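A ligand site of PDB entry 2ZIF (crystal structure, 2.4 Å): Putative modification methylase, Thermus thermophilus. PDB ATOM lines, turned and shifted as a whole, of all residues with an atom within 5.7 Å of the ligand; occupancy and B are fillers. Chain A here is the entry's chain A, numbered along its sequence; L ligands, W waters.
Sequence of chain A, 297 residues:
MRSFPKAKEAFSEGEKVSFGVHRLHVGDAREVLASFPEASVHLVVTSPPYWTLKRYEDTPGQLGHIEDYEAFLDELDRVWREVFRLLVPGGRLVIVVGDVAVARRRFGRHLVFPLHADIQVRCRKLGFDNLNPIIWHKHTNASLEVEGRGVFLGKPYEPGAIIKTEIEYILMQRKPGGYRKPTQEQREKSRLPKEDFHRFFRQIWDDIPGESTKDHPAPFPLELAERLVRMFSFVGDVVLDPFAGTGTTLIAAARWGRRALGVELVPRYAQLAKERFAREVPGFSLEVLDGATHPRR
Merely in contact with the ligand: Gly 27 (3.7 Å), Ser 47 (3.2 Å), Pro 48 (3.3 Å), Pro 49 (3.4 Å), Pro 219 (3.2 Å), Phe 220 (3.3 Å), Phe 243 (2.9 Å), Gly 247 (3.6 Å) and Val 266 (3.8 Å).
Water W1 lies within hydrogen-bond range of a nitrogen (N1) of the ligand (3.0 Å) and the backbone NH (N) of Phe 220 (3.1 Å).
An oxygen (O1) of the ligand lies close to the backbone NH (N) of Gly 245, at 3.5 Å. OD1 of Asp 28 lies within hydrogen-bond range of N4 of the ligand (2.5 Å). The backbone NH of Thr 246 is in hydrogen-bond range of an oxygen (O1) of the ligand (2.8 Å). N of Leu 265 lies close to N6 of the ligand (3.3 Å). The side-chain carboxylate (OE2) of Glu 264 is in hydrogen-bond range of an oxygen (O5) of the ligand, at 2.9 Å. The side-chain hydroxyl (OG1) of Thr 248 sits at hydrogen-bond distance from an oxygen (O2) of the ligand. The backbone carbonyl oxygen (O) of Ala 244 lies close to an oxygen (O1) of the ligand. N of Ala 29 is in hydrogen-bond range of N5 of the ligand.
The side-chain carboxylate of Glu 264 sits at hydrogen-bond distance from the backbone NH of Val 266 (3.2 Å). The backbone NH (N) of Ala 244 lies within hydrogen-bond range of the backbone carbonyl oxygen (O) of Val 263, at 2.9 Å. NE of Arg 276 sits at hydrogen-bond distance from OG1 of Thr 246, 3.1 Å away. The backbone carbonyl oxygen (O) of Glu 264 sits at hydrogen-bond distance from the backbone NH (N) of Gly 27 (2.9 Å). The backbone carbonyl oxygen (O) of Gly 27 lies close to the backbone NH (N) of Leu 265. The backbone NH (N) of Gly 245 is in hydrogen-bond range of the side-chain carboxylate (OE1) of Glu 264. The side-chain carboxylate of Asp 241 lies within hydrogen-bond range of the backbone NH of Phe 243. The guanidinium group of Arg 276 lies within hydrogen-bond range of the side-chain hydroxyl of Thr 248.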
ATOM      1  N   GLY A  27      21.367  -0.357   7.285  1.00  0.00           N
ATOM      2  CA  GLY A  27      21.478  -0.937   5.964  1.00  0.00           C
ATOM      3  C   GLY A  27      22.931  -1.196   5.619  1.00  0.00           C
ATOM      4  O   GLY A  27      23.817  -0.933   6.438  1.00  0.00           O
ATOM      5  N   ASP A  28      23.157  -1.716   4.425  1.00  0.00           N
ATOM      6  CA  ASP A  28      24.503  -2.012   3.951  1.00  0.00           C
ATOM      7  C   ASP A  28      25.229  -0.705   3.638  1.00  0.00           C
ATOM      8  O   ASP A  28      24.742   0.102   2.839  1.00  0.00           O
ATOM      9  CB  ASP A  28      24.420  -2.878   2.692  1.00  0.00           C
ATOM     10  CG  ASP A  28      25.778  -3.223   2.117  1.00  0.00           C
ATOM     11  OD1 ASP A  28      26.520  -3.978   2.769  1.00  0.00           O
ATOM     12  OD2 ASP A  28      26.095  -2.731   1.015  1.00  0.00           O
ATOM     13  N   ALA A  29      26.381  -0.492   4.272  1.00  0.00           N
ATOM     14  CA  ALA A  29      27.169   0.724   4.087  1.00  0.00           C
ATOM     15  C   ALA A  29      27.390   1.060   2.621  1.00  0.00           C
ATOM     16  O   ALA A  29      27.368   2.229   2.234  1.00  0.00           O
ATOM     17  CB  ALA A  29      28.507   0.584   4.790  1.00  0.00           C
ATOM     18  N   ARG A  30      27.607   0.039   1.802  1.00  0.00           N
ATOM     19  CA  ARG A  30      27.841   0.258   0.380  1.00  0.00           C
ATOM     20  C   ARG A  30      26.604   0.832  -0.306  1.00  0.00           C
ATOM     21  O   ARG A  30      26.716   1.725  -1.150  1.00  0.00           O
ATOM     22  CB  ARG A  30      28.245  -1.056  -0.298  1.00  0.00           C
ATOM     23  CG  ARG A  30      28.094  -1.057  -1.818  1.00  0.00           C
ATOM     24  CD  ARG A  30      28.769   0.157  -2.459  1.00  0.00           C
ATOM     25  NE  ARG A  30      28.576   0.223  -3.908  1.00  0.00           N
ATOM     26  CZ  ARG A  30      27.395   0.158  -4.514  1.00  0.00           C
ATOM     27  NH1 ARG A  30      26.275   0.025  -3.801  1.00  0.00           N
ATOM     28  NH2 ARG A  30      27.320   0.243  -5.833  1.00  0.00           N
ATOM     29  N   SER A  47      36.055   1.841  11.877  1.00  0.00           N
ATOM     30  CA  SER A  47      36.755   0.584  12.084  1.00  0.00           C
ATOM     31  C   SER A  47      36.080  -0.470  11.188  1.00  0.00           C
ATOM     32  O   SER A  47      34.911  -0.798  11.369  1.00  0.00           O
ATOM     33  CB  SER A  47      36.650   0.163  13.552  1.00  0.00           C
ATOM     34  OG  SER A  47      37.942  -0.029  14.090  1.00  0.00           O
ATOM     35  N   PRO A  48      36.814  -0.988  10.208  1.00  0.00           N
ATOM     36  CA  PRO A  48      36.248  -1.995   9.300  1.00  0.00           C
ATOM     37  C   PRO A  48      35.694  -3.218  10.047  1.00  0.00           C
ATOM     38  O   PRO A  48      36.229  -3.639  11.068  1.00  0.00           O
ATOM     39  CB  PRO A  48      37.418  -2.356   8.404  1.00  0.00           C
ATOM     40  CG  PRO A  48      38.605  -2.122   9.289  1.00  0.00           C
ATOM     41  CD  PRO A  48      38.257  -0.812   9.959  1.00  0.00           C
ATOM     42  N   PRO A  49      34.594  -3.792   9.536  1.00  0.00           N
ATOM     43  CA  PRO A  49      34.014  -4.963  10.176  1.00  0.00           C
ATOM     44  C   PRO A  49      34.994  -6.120  10.345  1.00  0.00           C
ATOM     45  O   PRO A  49      35.990  -6.230   9.630  1.00  0.00           O
ATOM     46  CB  PRO A  49      32.832  -5.316   9.278  1.00  0.00           C
ATOM     47  CG  PRO A  49      33.196  -4.709   7.948  1.00  0.00           C
ATOM     48  CD  PRO A  49      33.813  -3.397   8.350  1.00  0.00           C
ATOM     49  N   TYR A  50      34.703  -6.959  11.323  1.00  0.00           N
ATOM     50  CA  TYR A  50      35.506  -8.130  11.671  1.00  0.00           C
ATOM     51  C   TYR A  50      35.606  -9.095  10.491  1.00  0.00           C
ATOM     52  O   TYR A  50      34.626  -9.336   9.769  1.00  0.00           O
ATOM     53  CB  TYR A  50      34.855  -8.824  12.879  1.00  0.00           C
ATOM     54  CG  TYR A  50      35.699  -9.839  13.608  1.00  0.00           C
ATOM     55  CD1 TYR A  50      36.974  -9.505  14.098  1.00  0.00           C
ATOM     56  CD2 TYR A  50      35.206 -11.121  13.886  1.00  0.00           C
ATOM     57  CE1 TYR A  50      37.725 -10.420  14.840  1.00  0.00           C
ATOM     58  CE2 TYR A  50      35.949 -12.042  14.626  1.00  0.00           C
ATOM     59  CZ  TYR A  50      37.209 -11.681  15.097  1.00  0.00           C
ATOM     60  OH  TYR A  50      37.948 -12.578  15.837  1.00  0.00           O
ATOM     61  N   PRO A 219      35.148  -2.602  20.107  1.00  0.00           N
ATOM     62  CA  PRO A 219      34.994  -1.218  19.646  1.00  0.00           C
ATOM     63  C   PRO A 219      36.089  -0.329  20.240  1.00  0.00           C
ATOM     64  O   PRO A 219      36.479  -0.520  21.398  1.00  0.00           O
ATOM     65  CB  PRO A 219      33.600  -0.859  20.166  1.00  0.00           C
ATOM     66  CG  PRO A 219      33.580  -1.562  21.491  1.00  0.00           C
ATOM     67  CD  PRO A 219      34.180  -2.917  21.173  1.00  0.00           C
ATOM     68  N   PHE A 220      36.607   0.618  19.456  1.00  0.00           N
ATOM     69  CA  PHE A 220      37.643   1.487  19.992  1.00  0.00           C
ATOM     70  C   PHE A 220      37.021   2.410  21.030  1.00  0.00           C
ATOM     71  O   PHE A 220      35.810   2.641  21.014  1.00  0.00           O
ATOM     72  CB  PHE A 220      38.356   2.289  18.873  1.00  0.00           C
ATOM     73  CG  PHE A 220      37.436   2.944  17.858  1.00  0.00           C
ATOM     74  CD1 PHE A 220      36.550   3.946  18.240  1.00  0.00           C
ATOM     75  CD2 PHE A 220      37.517   2.596  16.517  1.00  0.00           C
ATOM     76  CE1 PHE A 220      35.746   4.596  17.289  1.00  0.00           C
ATOM     77  CE2 PHE A 220      36.719   3.240  15.562  1.00  0.00           C
ATOM     78  CZ  PHE A 220      35.834   4.237  15.952  1.00  0.00           C
ATOM     79  N   ASP A 241      30.555   7.548   9.914  1.00  0.00           N
ATOM     80  CA  ASP A 241      31.113   6.245  10.258  1.00  0.00           C
ATOM     81  C   ASP A 241      30.245   5.211   9.560  1.00  0.00           C
ATOM     82  O   ASP A 241      29.134   4.905  10.000  1.00  0.00           O
ATOM     83  CB  ASP A 241      31.088   5.975  11.768  1.00  0.00           C
ATOM     84  CG  ASP A 241      31.827   4.684  12.121  1.00  0.00           C
ATOM     85  OD1 ASP A 241      31.988   3.828  11.231  1.00  0.00           O
ATOM     86  OD2 ASP A 241      32.243   4.536  13.297  1.00  0.00           O
ATOM     87  N   PRO A 242      30.736   4.654   8.442  1.00  0.00           N
ATOM     88  CA  PRO A 242      30.040   3.651   7.629  1.00  0.00           C
ATOM     89  C   PRO A 242      29.700   2.372   8.403  1.00  0.00           C
ATOM     90  O   PRO A 242      28.779   1.638   8.020  1.00  0.00           O
ATOM     91  CB  PRO A 242      31.041   3.350   6.511  1.00  0.00           C
ATOM     92  CG  PRO A 242      31.887   4.551   6.447  1.00  0.00           C
ATOM     93  CD  PRO A 242      32.065   4.930   7.887  1.00  0.00           C
ATOM     94  N   PHE A 243      30.438   2.105   9.477  1.00  0.00           N
ATOM     95  CA  PHE A 243      30.239   0.912  10.299  1.00  0.00           C
ATOM     96  C   PHE A 243      30.050   1.331  11.753  1.00  0.00           C
ATOM     97  O   PHE A 243      30.832   0.972  12.622  1.00  0.00           O
ATOM     98  CB  PHE A 243      31.468  -0.007  10.188  1.00  0.00           C
ATOM     99  CG  PHE A 243      31.886  -0.286   8.776  1.00  0.00           C
ATOM    100  CD1 PHE A 243      33.086   0.228   8.269  1.00  0.00           C
ATOM    101  CD2 PHE A 243      31.084  -1.052   7.920  1.00  0.00           C
ATOM    102  CE1 PHE A 243      33.485  -0.005   6.948  1.00  0.00           C
ATOM    103  CE2 PHE A 243      31.453  -1.295   6.597  1.00  0.00           C
ATOM    104  CZ  PHE A 243      32.664  -0.767   6.107  1.00  0.00           C
ATOM    105  N   ALA A 244      28.971   2.079  11.990  1.00  0.00           N
ATOM    106  CA  ALA A 244      28.617   2.633  13.281  1.00  0.00           C
ATOM    107  C   ALA A 244      28.777   1.786  14.529  1.00  0.00           C
ATOM    108  O   ALA A 244      29.222   2.287  15.565  1.00  0.00           O
ATOM    109  CB  ALA A 244      27.199   3.186  13.217  1.00  0.00           C
ATOM    110  N   GLY A 245      28.387   0.502  14.462  1.00  0.00           N
ATOM    111  CA  GLY A 245      28.494  -0.351  15.636  1.00  0.00           C
ATOM    112  C   GLY A 245      27.631   0.204  16.759  1.00  0.00           C
ATOM    113  O   GLY A 245      26.445   0.430  16.559  1.00  0.00           O
ATOM    114  N   THR A 246      28.213   0.409  17.940  1.00  0.00           N
ATOM    115  CA  THR A 246      27.465   0.944  19.074  1.00  0.00           C
ATOM    116  C   THR A 246      27.472   2.477  19.045  1.00  0.00           C
ATOM    117  O   THR A 246      27.140   3.139  20.029  1.00  0.00           O
ATOM    118  CB  THR A 246      28.044   0.467  20.443  1.00  0.00           C
ATOM    119  OG1 THR A 246      29.334   1.057  20.663  1.00  0.00           O
ATOM    120  CG2 THR A 246      28.199  -1.053  20.450  1.00  0.00           C
ATOM    121  N   GLY A 247      27.886   3.022  17.903  1.00  0.00           N
ATOM    122  CA  GLY A 247      27.909   4.468  17.720  1.00  0.00           C
ATOM    123  C   GLY A 247      28.958   5.260  18.485  1.00  0.00           C
ATOM    124  O   GLY A 247      28.683   6.359  18.947  1.00  0.00           O
ATOM    125  N   THR A 248      30.152   4.702  18.637  1.00  0.00           N
ATOM    126  CA  THR A 248      31.222   5.384  19.347  1.00  0.00           C
ATOM    127  C   THR A 248      31.570   6.704  18.669  1.00  0.00           C
ATOM    128  O   THR A 248      31.644   7.740  19.309  1.00  0.00           O
ATOM    129  CB  THR A 248      32.483   4.518  19.402  1.00  0.00           C
ATOM    130  OG1 THR A 248      32.221   3.361  20.215  1.00  0.00           O
ATOM    131  CG2 THR A 248      33.656   5.291  19.988  1.00  0.00           C
ATOM    132  N   THR A 249      31.766   6.646  17.364  1.00  0.00           N
ATOM    133  CA  THR A 249      32.100   7.831  16.590  1.00  0.00           C
ATOM    134  C   THR A 249      30.977   8.873  16.626  1.00  0.00           C
ATOM    135  O   THR A 249      31.231  10.068  16.788  1.00  0.00           O
ATOM    136  CB  THR A 249      32.401   7.446  15.151  1.00  0.00           C
ATOM    137  OG1 THR A 249      33.486   6.533  15.135  1.00  0.00           O
ATOM    138  CG2 THR A 249      32.774   8.680  14.329  1.00  0.00           C
ATOM    139  N   VAL A 263      26.069   4.648   9.560  1.00  0.00           N
ATOM    140  CA  VAL A 263      25.411   3.558   8.857  1.00  0.00           C
ATOM    141  C   VAL A 263      25.796   2.281   9.600  1.00  0.00           C
ATOM    142  O   VAL A 263      26.968   2.093   9.942  1.00  0.00           O
ATOM    143  CB  VAL A 263      25.877   3.451   7.400  1.00  0.00           C
ATOM    144  CG1 VAL A 263      25.243   2.236   6.723  1.00  0.00           C
ATOM    145  CG2 VAL A 263      25.539   4.718   6.647  1.00  0.00           C
ATOM    146  N   GLU A 264      24.816   1.416   9.839  1.00  0.00           N
ATOM    147  CA  GLU A 264      25.044   0.151  10.515  1.00  0.00           C
ATOM    148  C   GLU A 264      24.129  -0.922   9.914  1.00  0.00           C
ATOM    149  O   GLU A 264      22.931  -0.704   9.734  1.00  0.00           O
ATOM    150  CB  GLU A 264      24.771   0.293  12.013  1.00  0.00           C
ATOM    151  CG  GLU A 264      24.860  -1.012  12.796  1.00  0.00           C
ATOM    152  CD  GLU A 264      26.141  -1.779  12.528  1.00  0.00           C
ATOM    153  OE1 GLU A 264      27.242  -1.266  12.866  1.00  0.00           O
ATOM    154  OE2 GLU A 264      26.060  -2.903  11.981  1.00  0.00           O
ATOM    155  N   LEU A 265      24.712  -2.067   9.586  1.00  0.00           N
ATOM    156  CA  LEU A 265      23.972  -3.179   8.970  1.00  0.00           C
ATOM    157  C   LEU A 265      22.934  -3.824   9.887  1.00  0.00           C
ATOM    158  O   LEU A 265      21.748  -3.834   9.586  1.00  0.00           O
ATOM    159  CB  LEU A 265      24.949  -4.258   8.509  1.00  0.00           C
ATOM    160  CG  LEU A 265      24.410  -5.464   7.738  1.00  0.00           C
ATOM    161  CD1 LEU A 265      23.786  -5.012   6.418  1.00  0.00           C
ATOM    162  CD2 LEU A 265      25.548  -6.445   7.462  1.00  0.00           C
ATOM    163  N   VAL A 266      23.396  -4.366  11.003  1.00  0.00           N
ATOM    164  CA  VAL A 266      22.520  -5.021  11.965  1.00  0.00           C
ATOM    165  C   VAL A 266      21.618  -4.052  12.711  1.00  0.00           C
ATOM    166  O   VAL A 266      22.087  -3.257  13.527  1.00  0.00           O
ATOM    167  CB  VAL A 266      23.347  -5.828  12.995  1.00  0.00           C
ATOM    168  CG1 VAL A 266      22.423  -6.569  13.954  1.00  0.00           C
ATOM    169  CG2 VAL A 266      24.268  -6.798  12.280  1.00  0.00           C
ATOM    170  N   TYR A 269      22.007  -3.571  16.590  1.00  0.00           N
ATOM    171  CA  TYR A 269      23.090  -2.706  17.052  1.00  0.00           C
ATOM    172  C   TYR A 269      22.744  -1.233  16.876  1.00  0.00           C
ATOM    173  O   TYR A 269      23.176  -0.374  17.650  1.00  0.00           O
ATOM    174  CB  TYR A 269      24.390  -3.016  16.299  1.00  0.00           C
ATOM    175  CG  TYR A 269      24.921  -4.414  16.534  1.00  0.00           C
ATOM    176  CD1 TYR A 269      24.848  -5.010  17.794  1.00  0.00           C
ATOM    177  CD2 TYR A 269      25.519  -5.138  15.493  1.00  0.00           C
ATOM    178  CE1 TYR A 269      25.364  -6.286  18.023  1.00  0.00           C
ATOM    179  CE2 TYR A 269      26.026  -6.415  15.711  1.00  0.00           C
ATOM    180  CZ  TYR A 269      25.943  -6.985  16.984  1.00  0.00           C
ATOM    181  OH  TYR A 269      26.459  -8.243  17.210  1.00  0.00           O
ATOM    182  N   ARG A 276      22.700   4.114  23.869  1.00  0.00           N
ATOM    183  CA  ARG A 276      24.035   4.446  24.329  1.00  0.00           C
ATOM    184  C   ARG A 276      24.292   5.913  24.019  1.00  0.00           C
ATOM    185  O   ARG A 276      24.942   6.621  24.787  1.00  0.00           O
ATOM    186  CB  ARG A 276      25.046   3.543  23.614  1.00  0.00           C
ATOM    187  CG  ARG A 276      26.501   3.878  23.851  1.00  0.00           C
ATOM    188  CD  ARG A 276      27.365   2.794  23.245  1.00  0.00           C
ATOM    189  NE  ARG A 276      28.688   3.254  22.821  1.00  0.00           N
ATOM    190  CZ  ARG A 276      29.584   3.813  23.625  1.00  0.00           C
ATOM    191  NH1 ARG A 276      30.756   4.190  23.134  1.00  0.00           N
ATOM    192  NH2 ARG A 276      29.305   4.003  24.902  1.00  0.00           N
HETATM  193  N1  LIG L   1      34.342   1.375  16.821  1.00  0.00           N
HETATM  194  C1  LIG L   1      32.999   1.136  16.261  1.00  0.00           C
HETATM  195  C2  LIG L   1      31.884   1.236  17.318  1.00  0.00           C
HETATM  196  O1  LIG L   1      30.722   1.028  16.965  1.00  0.00           O
HETATM  197  O2  LIG L   1      32.217   1.527  18.466  1.00  0.00           O
HETATM  198  C3  LIG L   1      32.884  -0.256  15.590  1.00  0.00           C
HETATM  199  C4  LIG L   1      32.367  -0.975  14.181  1.00  0.00           C
HETATM  200  S1  LIG L   1      32.672  -2.759  13.835  1.00  0.00           S
HETATM  201  C5  LIG L   1      34.494  -2.891  13.778  1.00  0.00           C
HETATM  202  C6  LIG L   1      32.061  -3.029  12.159  1.00  0.00           C
HETATM  203  C7  LIG L   1      30.529  -3.012  12.031  1.00  0.00           C
HETATM  204  O3  LIG L   1      30.133  -3.185  10.678  1.00  0.00           O
HETATM  205  C8  LIG L   1      29.773  -4.079  12.850  1.00  0.00           C
HETATM  206  O4  LIG L   1      28.977  -3.514  13.882  1.00  0.00           O
HETATM  207  C9  LIG L   1      29.073  -4.923  11.779  1.00  0.00           C
HETATM  208  O5  LIG L   1      27.737  -5.266  12.159  1.00  0.00           O
HETATM  209  C10 LIG L   1      28.948  -3.932  10.617  1.00  0.00           C
HETATM  210  N2  LIG L   1      28.906  -4.504   9.271  1.00  0.00           N
HETATM  211  C11 LIG L   1      29.388  -5.622   8.655  1.00  0.00           C
HETATM  212  N3  LIG L   1      29.164  -5.647   7.344  1.00  0.00           N
HETATM  213  C12 LIG L   1      28.491  -4.460   7.045  1.00  0.00           C
HETATM  214  C13 LIG L   1      27.970  -3.822   5.924  1.00  0.00           C
HETATM  215  N4  LIG L   1      28.052  -4.374   4.686  1.00  0.00           N
HETATM  216  N5  LIG L   1      27.340  -2.592   6.031  1.00  0.00           N
HETATM  217  C14 LIG L   1      27.235  -2.003   7.245  1.00  0.00           C
HETATM  218  N6  LIG L   1      27.719  -2.561   8.374  1.00  0.00           N
HETATM  219  C15 LIG L   1      28.334  -3.765   8.248  1.00  0.00           C
HETATM  220  O   HOH W   1      36.042  -1.086  16.950  1.00  0.00           O
